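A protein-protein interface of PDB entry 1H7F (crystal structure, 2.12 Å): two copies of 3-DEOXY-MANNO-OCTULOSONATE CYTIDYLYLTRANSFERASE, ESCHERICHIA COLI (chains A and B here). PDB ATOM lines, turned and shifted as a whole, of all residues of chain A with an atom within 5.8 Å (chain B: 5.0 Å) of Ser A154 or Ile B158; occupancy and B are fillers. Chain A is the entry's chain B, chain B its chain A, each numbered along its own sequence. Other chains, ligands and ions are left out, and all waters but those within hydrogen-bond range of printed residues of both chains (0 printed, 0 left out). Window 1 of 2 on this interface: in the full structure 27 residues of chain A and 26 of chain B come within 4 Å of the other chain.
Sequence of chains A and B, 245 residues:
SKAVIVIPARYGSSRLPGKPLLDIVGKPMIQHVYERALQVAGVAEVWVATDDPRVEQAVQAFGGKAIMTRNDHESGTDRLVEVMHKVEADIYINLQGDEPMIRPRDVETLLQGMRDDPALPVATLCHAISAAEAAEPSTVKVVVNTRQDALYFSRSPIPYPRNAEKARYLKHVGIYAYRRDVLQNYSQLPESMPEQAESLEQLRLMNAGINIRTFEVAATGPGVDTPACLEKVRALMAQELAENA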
ATOM      1  N   THR A 139      -4.974   3.100  23.866  1.00  0.00           N
ATOM      2  CA  THR A 139      -3.702   2.596  24.363  1.00  0.00           C
ATOM      3  C   THR A 139      -3.355   1.344  23.544  1.00  0.00           C
ATOM      4  O   THR A 139      -4.172   0.432  23.417  1.00  0.00           O
ATOM      5  CB  THR A 139      -3.815   2.243  25.860  1.00  0.00           C
ATOM      6  OG1 THR A 139      -3.816   3.447  26.629  1.00  0.00           O
ATOM      7  CG2 THR A 139      -2.666   1.399  26.313  1.00  0.00           C
ATOM      8  N   VAL A 140      -2.180   1.340  22.924  1.00  0.00           N
ATOM      9  CA  VAL A 140      -1.738   0.193  22.133  1.00  0.00           C
ATOM     10  C   VAL A 140      -0.976  -0.808  23.017  1.00  0.00           C
ATOM     11  O   VAL A 140       0.007  -0.451  23.673  1.00  0.00           O
ATOM     12  CB  VAL A 140      -0.837   0.637  20.953  1.00  0.00           C
ATOM     13  CG1 VAL A 140      -0.361  -0.574  20.164  1.00  0.00           C
ATOM     14  CG2 VAL A 140      -1.604   1.578  20.028  1.00  0.00           C
ATOM     15  N   LYS A 141      -1.482  -2.042  23.084  1.00  0.00           N
ATOM     16  CA  LYS A 141      -0.844  -3.111  23.869  1.00  0.00           C
ATOM     17  C   LYS A 141       0.095  -3.967  23.019  1.00  0.00           C
ATOM     18  O   LYS A 141      -0.089  -4.116  21.813  1.00  0.00           O
ATOM     19  CB  LYS A 141      -1.889  -4.016  24.529  1.00  0.00           C
ATOM     20  CG  LYS A 141      -2.506  -3.484  25.837  1.00  0.00           C
ATOM     21  CD  LYS A 141      -3.438  -2.296  25.602  1.00  0.00           C
ATOM     22  CE  LYS A 141      -4.591  -2.664  24.690  1.00  0.00           C
ATOM     23  NZ  LYS A 141      -5.586  -1.569  24.556  1.00  0.00           N
ATOM     24  N   VAL A 142       1.118  -4.518  23.660  1.00  0.00           N
ATOM     25  CA  VAL A 142       2.078  -5.368  22.974  1.00  0.00           C
ATOM     26  C   VAL A 142       2.337  -6.589  23.848  1.00  0.00           C
ATOM     27  O   VAL A 142       2.229  -6.506  25.076  1.00  0.00           O
ATOM     28  CB  VAL A 142       3.411  -4.602  22.662  1.00  0.00           C
ATOM     29  CG1 VAL A 142       4.115  -4.176  23.945  1.00  0.00           C
ATOM     30  CG2 VAL A 142       4.337  -5.448  21.804  1.00  0.00           C
ATOM     31  N   TYR A 152       2.594  -9.493  18.752  1.00  0.00           N
ATOM     32  CA  TYR A 152       1.528  -8.730  18.106  1.00  0.00           C
ATOM     33  C   TYR A 152       1.301  -7.424  18.871  1.00  0.00           C
ATOM     34  O   TYR A 152       1.636  -7.322  20.054  1.00  0.00           O
ATOM     35  CB  TYR A 152       0.229  -9.578  18.100  1.00  0.00           C
ATOM     36  CG  TYR A 152      -0.903  -9.020  17.256  1.00  0.00           C
ATOM     37  CD1 TYR A 152      -0.718  -8.738  15.907  1.00  0.00           C
ATOM     38  CD2 TYR A 152      -2.149  -8.747  17.820  1.00  0.00           C
ATOM     39  CE1 TYR A 152      -1.744  -8.192  15.144  1.00  0.00           C
ATOM     40  CE2 TYR A 152      -3.173  -8.203  17.064  1.00  0.00           C
ATOM     41  CZ  TYR A 152      -2.963  -7.924  15.734  1.00  0.00           C
ATOM     42  OH  TYR A 152      -3.969  -7.345  14.992  1.00  0.00           O
ATOM     43  N   PHE A 153       0.749  -6.431  18.175  1.00  0.00           N
ATOM     44  CA  PHE A 153       0.400  -5.126  18.756  1.00  0.00           C
ATOM     45  C   PHE A 153      -1.098  -4.971  18.532  1.00  0.00           C
ATOM     46  O   PHE A 153      -1.569  -5.134  17.408  1.00  0.00           O
ATOM     47  CB  PHE A 153       1.089  -3.985  18.004  1.00  0.00           C
ATOM     48  CG  PHE A 153       2.572  -3.926  18.194  1.00  0.00           C
ATOM     49  CD1 PHE A 153       3.420  -4.611  17.335  1.00  0.00           C
ATOM     50  CD2 PHE A 153       3.121  -3.139  19.188  1.00  0.00           C
ATOM     51  CE1 PHE A 153       4.801  -4.509  17.462  1.00  0.00           C
ATOM     52  CE2 PHE A 153       4.508  -3.029  19.325  1.00  0.00           C
ATOM     53  CZ  PHE A 153       5.343  -3.715  18.458  1.00  0.00           C
ATOM     54  N   SER A 154      -1.846  -4.597  19.562  1.00  0.00           N
ATOM     55  CA  SER A 154      -3.278  -4.458  19.376  1.00  0.00           C
ATOM     56  C   SER A 154      -3.942  -3.432  20.286  1.00  0.00           C
ATOM     57  O   SER A 154      -3.399  -3.049  21.325  1.00  0.00           O
ATOM     58  CB  SER A 154      -3.947  -5.820  19.594  1.00  0.00           C
ATOM     59  OG  SER A 154      -5.302  -5.820  19.178  1.00  0.00           O
ATOM     60  N   ARG A 155      -5.138  -3.006  19.887  1.00  0.00           N
ATOM     61  CA  ARG A 155      -5.932  -2.081  20.690  1.00  0.00           C
ATOM     62  C   ARG A 155      -6.797  -2.934  21.608  1.00  0.00           C
ATOM     63  O   ARG A 155      -7.341  -2.433  22.593  1.00  0.00           O
ATOM     64  CB  ARG A 155      -6.796  -1.170  19.812  1.00  0.00           C
ATOM     65  CG  ARG A 155      -5.978  -0.275  18.897  1.00  0.00           C
ATOM     66  CD  ARG A 155      -6.839   0.733  18.146  1.00  0.00           C
ATOM     67  NE  ARG A 155      -6.025   1.506  17.210  1.00  0.00           N
ATOM     68  CZ  ARG A 155      -5.309   2.577  17.551  1.00  0.00           C
ATOM     69  NH1 ARG A 155      -5.314   3.017  18.802  1.00  0.00           N
ATOM     70  NH2 ARG A 155      -4.529   3.160  16.654  1.00  0.00           N
ATOM     71  N   SER A 156      -6.926  -4.227  21.288  1.00  0.00           N
ATOM     72  CA  SER A 156      -7.692  -5.149  22.129  1.00  0.00           C
ATOM     73  C   SER A 156      -6.828  -5.460  23.340  1.00  0.00           C
ATOM     74  O   SER A 156      -5.609  -5.434  23.260  1.00  0.00           O
ATOM     75  CB  SER A 156      -7.983  -6.464  21.406  1.00  0.00           C
ATOM     76  OG  SER A 156      -8.910  -6.310  20.353  1.00  0.00           O
ATOM     77  N   PRO A 157      -7.446  -5.776  24.478  1.00  0.00           N
ATOM     78  CA  PRO A 157      -6.609  -6.076  25.634  1.00  0.00           C
ATOM     79  C   PRO A 157      -5.950  -7.448  25.469  1.00  0.00           C
ATOM     80  O   PRO A 157      -6.634  -8.468  25.583  1.00  0.00           O
ATOM     81  CB  PRO A 157      -7.617  -6.124  26.785  1.00  0.00           C
ATOM     82  CG  PRO A 157      -8.848  -5.446  26.248  1.00  0.00           C
ATOM     83  CD  PRO A 157      -8.870  -5.848  24.821  1.00  0.00           C
ATOM     84  N   ILE A 158      -4.668  -7.475  25.102  1.00  0.00           N
ATOM     85  CA  ILE A 158      -3.924  -8.737  24.984  1.00  0.00           C
ATOM     86  C   ILE A 158      -2.819  -8.691  26.028  1.00  0.00           C
ATOM     87  O   ILE A 158      -2.134  -7.679  26.166  1.00  0.00           O
ATOM     88  CB  ILE A 158      -3.304  -8.981  23.574  1.00  0.00           C
ATOM     89  CG1 ILE A 158      -2.422  -7.816  23.140  1.00  0.00           C
ATOM     90  CG2 ILE A 158      -4.392  -9.238  22.553  1.00  0.00           C
ATOM     91  CD1 ILE A 158      -1.873  -7.975  21.731  1.00  0.00           C
ATOM     92  N   GLU A 198      -6.798  -2.362  12.620  1.00  0.00           N
ATOM     93  CA  GLU A 198      -6.386  -1.825  13.916  1.00  0.00           C
ATOM     94  C   GLU A 198      -5.983  -0.367  13.814  1.00  0.00           C
ATOM     95  O   GLU A 198      -6.025   0.369  14.800  1.00  0.00           O
ATOM     96  CB  GLU A 198      -5.171  -2.603  14.427  1.00  0.00           C
ATOM     97  CG  GLU A 198      -5.425  -4.058  14.753  1.00  0.00           C
ATOM     98  CD  GLU A 198      -5.461  -4.317  16.239  1.00  0.00           C
ATOM     99  OE1 GLU A 198      -5.472  -3.343  17.016  1.00  0.00           O
ATOM    100  OE2 GLU A 198      -5.468  -5.505  16.641  1.00  0.00           O
ATOM    101  N   LEU A 200      -2.830   0.599  12.804  1.00  0.00           N
ATOM    102  CA  LEU A 200      -1.511   0.548  13.438  1.00  0.00           C
ATOM    103  C   LEU A 200      -0.497   0.244  12.350  1.00  0.00           C
ATOM    104  O   LEU A 200      -0.409  -0.888  11.872  1.00  0.00           O
ATOM    105  CB  LEU A 200      -1.476  -0.555  14.498  1.00  0.00           C
ATOM    106  CG  LEU A 200      -2.225  -0.276  15.801  1.00  0.00           C
ATOM    107  CD1 LEU A 200      -2.166  -1.477  16.706  1.00  0.00           C
ATOM    108  CD2 LEU A 200      -1.612   0.923  16.487  1.00  0.00           C
ATOM    109  N   LYS B 141      -9.039 -16.848  18.336  1.00  0.00           N
ATOM    110  CA  LYS B 141      -8.729 -16.136  17.102  1.00  0.00           C
ATOM    111  C   LYS B 141      -7.233 -16.187  16.842  1.00  0.00           C
ATOM    112  O   LYS B 141      -6.436 -16.311  17.771  1.00  0.00           O
ATOM    113  CB  LYS B 141      -9.180 -14.663  17.189  1.00  0.00           C
ATOM    114  CG  LYS B 141     -10.672 -14.400  16.918  1.00  0.00           C
ATOM    115  CD  LYS B 141     -11.580 -14.946  18.004  1.00  0.00           C
ATOM    116  CE  LYS B 141     -11.333 -14.288  19.330  1.00  0.00           C
ATOM    117  NZ  LYS B 141     -12.289 -14.760  20.367  1.00  0.00           N
ATOM    118  N   VAL B 142      -6.854 -16.053  15.575  1.00  0.00           N
ATOM    119  CA  VAL B 142      -5.461 -16.073  15.202  1.00  0.00           C
ATOM    120  C   VAL B 142      -5.248 -15.066  14.085  1.00  0.00           C
ATOM    121  O   VAL B 142      -6.129 -14.861  13.261  1.00  0.00           O
ATOM    122  CB  VAL B 142      -5.015 -17.504  14.744  1.00  0.00           C
ATOM    123  CG1 VAL B 142      -5.815 -17.979  13.515  1.00  0.00           C
ATOM    124  CG2 VAL B 142      -3.523 -17.518  14.433  1.00  0.00           C
ATOM    125  N   VAL B 143      -4.095 -14.398  14.106  1.00  0.00           N
ATOM    126  CA  VAL B 143      -3.730 -13.432  13.081  1.00  0.00           C
ATOM    127  C   VAL B 143      -2.449 -13.969  12.483  1.00  0.00           C
ATOM    128  O   VAL B 143      -1.566 -14.380  13.220  1.00  0.00           O
ATOM    129  CB  VAL B 143      -3.458 -12.031  13.684  1.00  0.00           C
ATOM    130  CG1 VAL B 143      -2.931 -11.097  12.607  1.00  0.00           C
ATOM    131  CG2 VAL B 143      -4.737 -11.453  14.259  1.00  0.00           C
ATOM    132  N   TYR B 152      -0.105 -14.251  16.667  1.00  0.00           N
ATOM    133  CA  TYR B 152      -0.586 -14.422  18.027  1.00  0.00           C
ATOM    134  C   TYR B 152      -1.920 -15.151  17.973  1.00  0.00           C
ATOM    135  O   TYR B 152      -2.559 -15.189  16.927  1.00  0.00           O
ATOM    136  CB  TYR B 152      -0.769 -13.043  18.684  1.00  0.00           C
ATOM    137  CG  TYR B 152      -1.064 -13.079  20.165  1.00  0.00           C
ATOM    138  CD1 TYR B 152      -0.169 -13.661  21.055  1.00  0.00           C
ATOM    139  CD2 TYR B 152      -2.249 -12.561  20.677  1.00  0.00           C
ATOM    140  CE1 TYR B 152      -0.446 -13.738  22.405  1.00  0.00           C
ATOM    141  CE2 TYR B 152      -2.533 -12.635  22.048  1.00  0.00           C
ATOM    142  CZ  TYR B 152      -1.627 -13.227  22.897  1.00  0.00           C
ATOM    143  OH  TYR B 152      -1.896 -13.337  24.251  1.00  0.00           O
ATOM    144  N   PHE B 153      -2.311 -15.748  19.097  1.00  0.00           N
ATOM    145  CA  PHE B 153      -3.581 -16.468  19.238  1.00  0.00           C
ATOM    146  C   PHE B 153      -4.209 -15.833  20.453  1.00  0.00           C
ATOM    147  O   PHE B 153      -3.536 -15.683  21.464  1.00  0.00           O
ATOM    148  CB  PHE B 153      -3.383 -17.960  19.596  1.00  0.00           C
ATOM    149  CG  PHE B 153      -2.822 -18.800  18.485  1.00  0.00           C
ATOM    150  CD1 PHE B 153      -1.456 -18.881  18.281  1.00  0.00           C
ATOM    151  CD2 PHE B 153      -3.664 -19.524  17.657  1.00  0.00           C
ATOM    152  CE1 PHE B 153      -0.930 -19.671  17.260  1.00  0.00           C
ATOM    153  CE2 PHE B 153      -3.152 -20.315  16.637  1.00  0.00           C
ATOM    154  CZ  PHE B 153      -1.778 -20.386  16.439  1.00  0.00           C
ATOM    155  N   SER B 154      -5.506 -15.540  20.408  1.00  0.00           N
ATOM    156  CA  SER B 154      -6.142 -14.925  21.568  1.00  0.00           C
ATOM    157  C   SER B 154      -7.638 -15.143  21.641  1.00  0.00           C
ATOM    158  O   SER B 154      -8.282 -15.447  20.642  1.00  0.00           O
ATOM    159  CB  SER B 154      -5.870 -13.408  21.569  1.00  0.00           C
ATOM    160  OG  SER B 154      -6.357 -12.793  22.753  1.00  0.00           O
ATOM    161  N   SER B 156      -9.371 -12.692  22.844  1.00  0.00           N
ATOM    162  CA  SER B 156      -9.789 -11.309  22.576  1.00  0.00           C
ATOM    163  C   SER B 156      -9.981 -11.190  21.071  1.00  0.00           C
ATOM    164  O   SER B 156      -9.280 -11.833  20.296  1.00  0.00           O
ATOM    165  CB  SER B 156      -8.693 -10.309  22.969  1.00  0.00           C
ATOM    166  OG  SER B 156      -8.621 -10.101  24.367  1.00  0.00           O
ATOM    167  N   PRO B 157     -10.948 -10.372  20.628  1.00  0.00           N
ATOM    168  CA  PRO B 157     -11.100 -10.276  19.181  1.00  0.00           C
ATOM    169  C   PRO B 157      -9.895  -9.589  18.570  1.00  0.00           C
ATOM    170  O   PRO B 157      -9.580  -8.452  18.921  1.00  0.00           O
ATOM    171  CB  PRO B 157     -12.360  -9.418  19.031  1.00  0.00           C
ATOM    172  CG  PRO B 157     -13.147  -9.774  20.256  1.00  0.00           C
ATOM    173  CD  PRO B 157     -12.085  -9.739  21.318  1.00  0.00           C
ATOM    174  N   ILE B 158      -9.163 -10.302  17.724  1.00  0.00           N
ATOM    175  CA  ILE B 158      -8.025  -9.711  17.035  1.00  0.00           C
ATOM    176  C   ILE B 158      -8.190 -10.073  15.569  1.00  0.00           C
ATOM    177  O   ILE B 158      -8.604 -11.176  15.249  1.00  0.00           O
ATOM    178  CB  ILE B 158      -6.637 -10.200  17.577  1.00  0.00           C
ATOM    179  CG1 ILE B 158      -6.550 -11.733  17.577  1.00  0.00           C
ATOM    180  CG2 ILE B 158      -6.391  -9.645  18.978  1.00  0.00           C
ATOM    181  CD1 ILE B 158      -5.168 -12.271  17.967  1.00  0.00           C
ATOM    182  N   PRO B 159      -7.936  -9.127  14.658  1.00  0.00           N
ATOM    183  CA  PRO B 159      -7.507  -7.750  14.918  1.00  0.00           C
ATOM    184  C   PRO B 159      -8.625  -6.914  15.550  1.00  0.00           C
ATOM    185  O   PRO B 159      -9.814  -7.246  15.417  1.00  0.00           O
ATOM    186  CB  PRO B 159      -7.140  -7.254  13.521  1.00  0.00           C
ATOM    187  CG  PRO B 159      -8.094  -7.989  12.649  1.00  0.00           C
ATOM    188  CD  PRO B 159      -8.051  -9.376  13.211  1.00  0.00           C
ATOM    189  N   TYR B 160      -8.249  -5.893  16.321  1.00  0.00           N
ATOM    190  CA  TYR B 160      -9.246  -5.023  16.950  1.00  0.00           C
ATOM    191  C   TYR B 160      -9.998  -4.341  15.812  1.00  0.00           C
ATOM    192  O   TYR B 160      -9.405  -3.954  14.813  1.00  0.00           O
ATOM    193  CB  TYR B 160      -8.573  -3.982  17.848  1.00  0.00           C
ATOM    194  CG  TYR B 160      -9.559  -3.067  18.525  1.00  0.00           C
ATOM    195  CD1 TYR B 160     -10.196  -3.454  19.696  1.00  0.00           C
ATOM    196  CD2 TYR B 160      -9.899  -1.838  17.960  1.00  0.00           C
ATOM    197  CE1 TYR B 160     -11.152  -2.649  20.287  1.00  0.00           C
ATOM    198  CE2 TYR B 160     -10.858  -1.025  18.544  1.00  0.00           C
ATOM    199  CZ  TYR B 160     -11.482  -1.438  19.703  1.00  0.00           C
ATOM    200  OH  TYR B 160     -12.467  -0.661  20.269  1.00  0.00           O
ATOM    201  N   TYR B 169     -11.744 -12.065  10.293  1.00  0.00           N
ATOM    202  CA  TYR B 169     -11.430 -12.948  11.409  1.00  0.00           C
ATOM    203  C   TYR B 169     -11.178 -14.401  11.035  1.00  0.00           C
ATOM    204  O   TYR B 169     -11.808 -14.937  10.125  1.00  0.00           O
ATOM    205  CB  TYR B 169     -12.527 -12.869  12.466  1.00  0.00           C
ATOM    206  CG  TYR B 169     -12.573 -11.528  13.137  1.00  0.00           C
ATOM    207  CD1 TYR B 169     -11.747 -11.249  14.220  1.00  0.00           C
ATOM    208  CD2 TYR B 169     -13.389 -10.511  12.649  1.00  0.00           C
ATOM    209  CE1 TYR B 169     -11.723  -9.990  14.799  1.00  0.00           C
ATOM    210  CE2 TYR B 169     -13.372  -9.242  13.220  1.00  0.00           C
ATOM    211  CZ  TYR B 169     -12.538  -8.989  14.293  1.00  0.00           C
ATOM    212  OH  TYR B 169     -12.504  -7.736  14.862  1.00  0.00           O
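The backbone carbonyl oxygen (O) of Pro A157 sits at hydrogen-bond distance from the side-chain hydroxyl (OG) of Ser B156, 2.8 Å away. The side-chain hydroxyl of Ser A156 sits at hydrogen-bond distance from the backbone carbonyl oxygen of Pro B157 (2.7 Å). N of Tyr B160 is in hydrogen-bond range of OE2 of Glu A198 (2.8 Å).
Of the 12 printed residues of chain B, 6 touch a printed residue of chain A. Hydrophobic or aromatic side chains of chain B within 4 Å of the printed part of chain A: Tyr B152, Ile B158, Pro B159 and Tyr B160. Along chain B the printed residues that touch a printed residue of chain A span positions 152 to 160. Among the printed residues, no Asp or Glu carboxylate lies within 4 Å of a Lys or Arg side-chain nitrogen of the other chain.
Of the printed residues of chain B, Ser A154 touches Ile B158 (3.98 Å) and Tyr B160 (3.98 Å). Of the printed residues of chain B, Glu A198 touches Pro B159 (3.5 Å) and Tyr B160 (2.8 Å). Of the printed residues of chain A, Tyr B152 touches Tyr A152 and Ile A158. Ser B154 touches none of the printed residues of chain A. Of the printed residues of chain A, Ser B156 touches Pro A157. Of the printed residues of chain A, Pro B157 touches Ser A156. Of the printed residues of chain A, Ile B158 touches Ser A154 (3.98 Å). Tyr B169 touches none of the printed residues of chain A. The nearest printed residue of chain B that does not touch Ser A154 is Pro B157 (5.0 Å).
Among the printed residues, pairs that only touch across the chains: Tyr A152 with Tyr B152, Tyr A152 with Pro B159, Ser A154 with Ile B158, Ser A154 with Tyr B160, Arg A155 with Tyr B160, Ser A156 with Tyr B160, Ile A158 with Tyr B152 and Glu A198 with Pro B159.
Tyr A152 touches its own counterpart, Tyr B152. Ser A154 touches Ile B158, but with the chains exchanged Ile A158 does not touch Ser B154 (4.1 Å). Ser A156 touches Pro B157, and with the chains exchanged Pro A157 touches Ser B156. Ile A158 touches Tyr B152, but with the chains exchanged Tyr A152 does not touch Ile B158 (4.01 Å). Of the 11 pairs that touch across the chains among the printed residues, 3 have their exchanged pair printed and touching as well.
The backbone NH of Val B143 sits at hydrogen-bond distance from the backbone carbonyl oxygen of Tyr B152, 3.3 Å away. The side-chain hydroxyl (OG) of Ser B154 sits at hydrogen-bond distance from the backbone NH (N) of Ser B156, at 3.0 Å. The backbone carbonyl oxygen (O) of Pro B159 sits at hydrogen-bond distance from the side-chain hydroxyl (OH) of Tyr B169 (2.8 Å). The side-chain amino group (NZ) of Lys A141 sits at hydrogen-bond distance from the backbone carbonyl oxygen (O) of Arg A155. The side-chain hydroxyl of Tyr A152 sits at hydrogen-bond distance from the side-chain carboxylate of Glu A198. The side-chain hydroxyl of Ser A154 is in hydrogen-bond range of the backbone NH of Ser A156, at 3.1 Å.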
